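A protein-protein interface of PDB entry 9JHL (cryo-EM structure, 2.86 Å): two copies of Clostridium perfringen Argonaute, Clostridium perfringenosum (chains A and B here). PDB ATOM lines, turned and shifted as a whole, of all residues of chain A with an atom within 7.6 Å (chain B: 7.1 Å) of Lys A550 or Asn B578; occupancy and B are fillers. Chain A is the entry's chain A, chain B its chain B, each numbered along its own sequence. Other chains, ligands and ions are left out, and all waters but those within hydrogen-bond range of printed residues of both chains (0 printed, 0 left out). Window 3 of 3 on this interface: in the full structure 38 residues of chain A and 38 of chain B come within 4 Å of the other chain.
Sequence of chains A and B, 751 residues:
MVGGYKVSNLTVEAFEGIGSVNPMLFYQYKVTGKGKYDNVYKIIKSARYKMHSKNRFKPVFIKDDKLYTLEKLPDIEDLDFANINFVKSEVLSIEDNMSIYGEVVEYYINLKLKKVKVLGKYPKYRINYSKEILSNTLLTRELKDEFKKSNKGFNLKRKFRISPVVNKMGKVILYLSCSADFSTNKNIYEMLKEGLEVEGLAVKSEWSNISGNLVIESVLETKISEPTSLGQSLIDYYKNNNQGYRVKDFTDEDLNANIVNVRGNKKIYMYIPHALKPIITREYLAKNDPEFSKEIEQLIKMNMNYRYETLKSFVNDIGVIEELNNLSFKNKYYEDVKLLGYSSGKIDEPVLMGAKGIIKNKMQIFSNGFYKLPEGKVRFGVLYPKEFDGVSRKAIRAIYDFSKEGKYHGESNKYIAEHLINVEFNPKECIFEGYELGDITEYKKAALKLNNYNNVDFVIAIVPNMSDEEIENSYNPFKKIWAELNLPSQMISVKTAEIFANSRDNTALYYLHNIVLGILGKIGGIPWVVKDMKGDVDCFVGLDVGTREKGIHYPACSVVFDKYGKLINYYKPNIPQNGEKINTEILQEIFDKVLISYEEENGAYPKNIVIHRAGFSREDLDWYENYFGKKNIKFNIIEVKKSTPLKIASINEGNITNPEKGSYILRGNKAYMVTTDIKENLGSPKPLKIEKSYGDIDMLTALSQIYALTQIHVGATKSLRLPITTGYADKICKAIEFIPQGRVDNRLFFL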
ATOM      1  N   SER A 211     -37.569   7.082   9.345  1.00  0.00           N
ATOM      2  CA  SER A 211     -38.251   7.588   8.161  1.00  0.00           C
ATOM      3  C   SER A 211     -37.329   7.424   6.957  1.00  0.00           C
ATOM      4  O   SER A 211     -36.347   8.159   6.813  1.00  0.00           O
ATOM      5  CB  SER A 211     -38.659   9.047   8.350  1.00  0.00           C
ATOM      6  OG  SER A 211     -37.525   9.886   8.450  1.00  0.00           O
ATOM      7  N   THR A 547     -36.235  22.347  -1.676  1.00  0.00           N
ATOM      8  CA  THR A 547     -35.464  21.208  -1.190  1.00  0.00           C
ATOM      9  C   THR A 547     -35.828  20.007  -2.053  1.00  0.00           C
ATOM     10  O   THR A 547     -36.923  19.456  -1.927  1.00  0.00           O
ATOM     11  CB  THR A 547     -35.746  20.940   0.284  1.00  0.00           C
ATOM     12  OG1 THR A 547     -37.122  20.576   0.452  1.00  0.00           O
ATOM     13  CG2 THR A 547     -35.468  22.181   1.109  1.00  0.00           C
ATOM     14  N   ARG A 548     -34.906  19.598  -2.927  1.00  0.00           N
ATOM     15  CA  ARG A 548     -35.182  18.480  -3.822  1.00  0.00           C
ATOM     16  C   ARG A 548     -35.202  17.162  -3.054  1.00  0.00           C
ATOM     17  O   ARG A 548     -36.166  16.392  -3.147  1.00  0.00           O
ATOM     18  CB  ARG A 548     -34.144  18.452  -4.947  1.00  0.00           C
ATOM     19  CG  ARG A 548     -34.523  17.617  -6.170  1.00  0.00           C
ATOM     20  CD  ARG A 548     -34.014  16.190  -6.146  1.00  0.00           C
ATOM     21  NE  ARG A 548     -32.560  16.116  -6.041  1.00  0.00           N
ATOM     22  CZ  ARG A 548     -31.740  16.189  -7.082  1.00  0.00           C
ATOM     23  NH1 ARG A 548     -32.239  16.335  -8.299  1.00  0.00           N
ATOM     24  NH2 ARG A 548     -30.427  16.109  -6.908  1.00  0.00           N
ATOM     25  N   GLU A 549     -34.150  16.888  -2.284  1.00  0.00           N
ATOM     26  CA  GLU A 549     -34.061  15.680  -1.473  1.00  0.00           C
ATOM     27  C   GLU A 549     -33.446  16.032  -0.126  1.00  0.00           C
ATOM     28  O   GLU A 549     -33.344  17.203   0.251  1.00  0.00           O
ATOM     29  CB  GLU A 549     -33.242  14.588  -2.170  1.00  0.00           C
ATOM     30  CG  GLU A 549     -33.950  13.895  -3.314  1.00  0.00           C
ATOM     31  CD  GLU A 549     -33.070  12.882  -4.011  1.00  0.00           C
ATOM     32  OE1 GLU A 549     -31.861  12.830  -3.702  1.00  0.00           O
ATOM     33  OE2 GLU A 549     -33.590  12.132  -4.864  1.00  0.00           O
ATOM     34  N   LYS A 550     -33.045  14.995   0.604  1.00  0.00           N
ATOM     35  CA  LYS A 550     -32.361  15.177   1.874  1.00  0.00           C
ATOM     36  C   LYS A 550     -30.947  15.683   1.634  1.00  0.00           C
ATOM     37  O   LYS A 550     -30.164  15.051   0.920  1.00  0.00           O
ATOM     38  CB  LYS A 550     -32.329  13.859   2.645  1.00  0.00           C
ATOM     39  CG  LYS A 550     -31.729  13.957   4.032  1.00  0.00           C
ATOM     40  CD  LYS A 550     -31.864  12.636   4.767  1.00  0.00           C
ATOM     41  CE  LYS A 550     -31.344  12.730   6.187  1.00  0.00           C
ATOM     42  NZ  LYS A 550     -31.505  11.437   6.907  1.00  0.00           N
ATOM     43  N   GLY A 551     -30.622  16.832   2.222  1.00  0.00           N
ATOM     44  CA  GLY A 551     -29.304  17.410   2.065  1.00  0.00           C
ATOM     45  C   GLY A 551     -29.062  18.120   0.754  1.00  0.00           C
ATOM     46  O   GLY A 551     -27.961  18.642   0.547  1.00  0.00           O
ATOM     47  N   ILE A 552     -30.048  18.157  -0.136  1.00  0.00           N
ATOM     48  CA  ILE A 552     -29.952  18.854  -1.410  1.00  0.00           C
ATOM     49  C   ILE A 552     -30.968  19.982  -1.389  1.00  0.00           C
ATOM     50  O   ILE A 552     -32.152  19.750  -1.128  1.00  0.00           O
ATOM     51  CB  ILE A 552     -30.222  17.914  -2.596  1.00  0.00           C
ATOM     52  CG1 ILE A 552     -29.258  16.734  -2.587  1.00  0.00           C
ATOM     53  CG2 ILE A 552     -30.103  18.664  -3.904  1.00  0.00           C
ATOM     54  CD1 ILE A 552     -29.656  15.627  -3.543  1.00  0.00           C
ATOM     55  N   HIS A 553     -30.507  21.197  -1.651  1.00  0.00           N
ATOM     56  CA  HIS A 553     -31.380  22.353  -1.777  1.00  0.00           C
ATOM     57  C   HIS A 553     -31.305  22.849  -3.210  1.00  0.00           C
ATOM     58  O   HIS A 553     -30.230  22.830  -3.815  1.00  0.00           O
ATOM     59  CB  HIS A 553     -30.972  23.458  -0.801  1.00  0.00           C
ATOM     60  CG  HIS A 553     -31.198  23.107   0.634  1.00  0.00           C
ATOM     61  ND1 HIS A 553     -30.305  22.355   1.364  1.00  0.00           N
ATOM     62  CD2 HIS A 553     -32.204  23.423   1.482  1.00  0.00           C
ATOM     63  CE1 HIS A 553     -30.760  22.204   2.594  1.00  0.00           C
ATOM     64  NE2 HIS A 553     -31.913  22.843   2.692  1.00  0.00           N
ATOM     65  N   VAL B 545     -16.240  16.004  -7.224  1.00  0.00           N
ATOM     66  CA  VAL B 545     -17.281  16.671  -6.455  1.00  0.00           C
ATOM     67  C   VAL B 545     -16.586  17.382  -5.312  1.00  0.00           C
ATOM     68  O   VAL B 545     -15.884  16.745  -4.518  1.00  0.00           O
ATOM     69  CB  VAL B 545     -18.329  15.692  -5.907  1.00  0.00           C
ATOM     70  CG1 VAL B 545     -19.380  16.439  -5.114  1.00  0.00           C
ATOM     71  CG2 VAL B 545     -18.957  14.929  -7.010  1.00  0.00           C
ATOM     72  N   GLY B 551     -22.695  20.951   4.427  1.00  0.00           N
ATOM     73  CA  GLY B 551     -23.980  20.730   3.802  1.00  0.00           C
ATOM     74  C   GLY B 551     -24.116  21.268   2.397  1.00  0.00           C
ATOM     75  O   GLY B 551     -25.185  21.117   1.796  1.00  0.00           O
ATOM     76  N   HIS B 553     -22.426  21.041  -1.402  1.00  0.00           N
ATOM     77  CA  HIS B 553     -21.512  20.357  -2.303  1.00  0.00           C
ATOM     78  C   HIS B 553     -21.479  21.121  -3.614  1.00  0.00           C
ATOM     79  O   HIS B 553     -22.514  21.624  -4.062  1.00  0.00           O
ATOM     80  CB  HIS B 553     -21.948  18.909  -2.533  1.00  0.00           C
ATOM     81  CG  HIS B 553     -21.827  18.045  -1.320  1.00  0.00           C
ATOM     82  ND1 HIS B 553     -22.788  18.009  -0.334  1.00  0.00           N
ATOM     83  CD2 HIS B 553     -20.868  17.167  -0.942  1.00  0.00           C
ATOM     84  CE1 HIS B 553     -22.417  17.160   0.609  1.00  0.00           C
ATOM     85  NE2 HIS B 553     -21.254  16.638   0.264  1.00  0.00           N
ATOM     86  N   PRO B 576     -27.326  20.283  -7.521  1.00  0.00           N
ATOM     87  CA  PRO B 576     -26.348  19.770  -6.559  1.00  0.00           C
ATOM     88  C   PRO B 576     -26.769  18.385  -6.101  1.00  0.00           C
ATOM     89  O   PRO B 576     -27.890  17.945  -6.363  1.00  0.00           O
ATOM     90  CB  PRO B 576     -26.412  20.783  -5.412  1.00  0.00           C
ATOM     91  CG  PRO B 576     -27.801  21.289  -5.471  1.00  0.00           C
ATOM     92  CD  PRO B 576     -28.187  21.318  -6.926  1.00  0.00           C
ATOM     93  N   GLN B 577     -25.872  17.693  -5.417  1.00  0.00           N
ATOM     94  CA  GLN B 577     -26.211  16.360  -4.959  1.00  0.00           C
ATOM     95  C   GLN B 577     -25.873  16.189  -3.485  1.00  0.00           C
ATOM     96  O   GLN B 577     -25.257  17.050  -2.854  1.00  0.00           O
ATOM     97  CB  GLN B 577     -25.504  15.306  -5.803  1.00  0.00           C
ATOM     98  CG  GLN B 577     -24.009  15.271  -5.647  1.00  0.00           C
ATOM     99  CD  GLN B 577     -23.386  14.294  -6.602  1.00  0.00           C
ATOM    100  OE1 GLN B 577     -24.063  13.724  -7.452  1.00  0.00           O
ATOM    101  NE2 GLN B 577     -22.106  14.047  -6.434  1.00  0.00           N
ATOM    102  N   ASN B 578     -26.310  15.063  -2.935  1.00  0.00           N
ATOM    103  CA  ASN B 578     -26.091  14.746  -1.532  1.00  0.00           C
ATOM    104  C   ASN B 578     -24.847  13.877  -1.431  1.00  0.00           C
ATOM    105  O   ASN B 578     -24.938  12.646  -1.467  1.00  0.00           O
ATOM    106  CB  ASN B 578     -27.304  14.032  -0.938  1.00  0.00           C
ATOM    107  CG  ASN B 578     -27.255  13.948   0.579  1.00  0.00           C
ATOM    108  OD1 ASN B 578     -26.327  14.447   1.218  1.00  0.00           O
ATOM    109  ND2 ASN B 578     -28.259  13.307   1.164  1.00  0.00           N
ATOM    110  N   GLY B 579     -23.696  14.511  -1.304  1.00  0.00           N
ATOM    111  CA  GLY B 579     -22.487  13.773  -1.039  1.00  0.00           C
ATOM    112  C   GLY B 579     -21.464  13.813  -2.148  1.00  0.00           C
ATOM    113  O   GLY B 579     -21.578  14.521  -3.151  1.00  0.00           O
ATOM    114  N   GLU B 580     -20.426  13.013  -1.935  1.00  0.00           N
ATOM    115  CA  GLU B 580     -19.269  12.940  -2.807  1.00  0.00           C
ATOM    116  C   GLU B 580     -19.384  11.826  -3.834  1.00  0.00           C
ATOM    117  O   GLU B 580     -18.502  11.688  -4.686  1.00  0.00           O
ATOM    118  CB  GLU B 580     -18.011  12.756  -1.961  1.00  0.00           C
ATOM    119  CG  GLU B 580     -17.704  13.949  -1.072  1.00  0.00           C
ATOM    120  CD  GLU B 580     -16.552  13.691  -0.125  1.00  0.00           C
ATOM    121  OE1 GLU B 580     -16.115  12.527  -0.027  1.00  0.00           O
ATOM    122  OE2 GLU B 580     -16.078  14.653   0.517  1.00  0.00           O
ATOM    123  N   LYS B 581     -20.445  11.031  -3.771  1.00  0.00           N
ATOM    124  CA  LYS B 581     -20.735  10.017  -4.773  1.00  0.00           C
ATOM    125  C   LYS B 581     -21.590  10.636  -5.866  1.00  0.00           C
ATOM    126  O   LYS B 581     -22.587  11.304  -5.576  1.00  0.00           O
ATOM    127  CB  LYS B 581     -21.462   8.822  -4.155  1.00  0.00           C
ATOM    128  CG  LYS B 581     -21.746   7.699  -5.130  1.00  0.00           C
ATOM    129  CD  LYS B 581     -22.409   6.522  -4.445  1.00  0.00           C
ATOM    130  CE  LYS B 581     -22.689   5.405  -5.434  1.00  0.00           C
ATOM    131  NZ  LYS B 581     -23.289   4.213  -4.781  1.00  0.00           N
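The guanidinium group (NH2) of Arg A548 sits at hydrogen-bond distance from the backbone carbonyl oxygen (O) of Pro B576 (3.2 Å). The backbone carbonyl oxygen of Lys A550 lies within hydrogen-bond range of the side-chain amide nitrogen of Asn B578 (2.6 Å).
NE2 of Gln B577 is in hydrogen-bond range of O of Gly B579 (3.4 Å). NE2 of Gln B577 is in hydrogen-bond range of O of Lys B581.
Gly B551 touches Gly A551 (O to O, 3.9 Å). Ile A552 touches Pro B576 (CG2 to O, 3.4 Å). Gln B577 touches Ile A552 (C to CG1, 3.5 Å). N of Asn B578 touches CG1 of Ile A552 (3.4 Å). Pro B576 touches His A553 (CG to O, 3.3 Å).
Of the printed residues of chain B, Arg A548 touches Pro B576 (3.2 Å). Glu A549 touches none of the printed residues of chain B. Of the printed residues of chain B, Gly A551 touches Gly B551. Printed residues of chain B within 4 Å of Ile A552: Pro B576 (3.4 Å), Gln B577 (3.5 Å) and Asn B578 (3.4 Å). Val B545 touches none of the printed residues of chain A. Printed residues of chain A within 4 Å of Gly B551: Gly A551. Of the printed residues of chain A, Gln B577 touches Ile A552 (3.5 Å). Asn B578 touches just these residues of chain A: Lys A550 and Ile A552. The nearest residue of chain A that does not touch Asn B578 is Gly A551 (4.3 Å). The nearest printed residue of chain B that does not touch Gly A551 is Asn B578 (4.3 Å).
Of the 8 printed residues of chain A, 5 touch a printed residue of chain B. Hydrophobic or aromatic side chains of chain A that line the printed part of chain B: Ile A552. Of the 9 printed residues of chain B, 4 touch a printed residue of chain A. Among the printed residues, 7 pairs touch across the chains.
Gly A551 touches its own counterpart, Gly B551.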
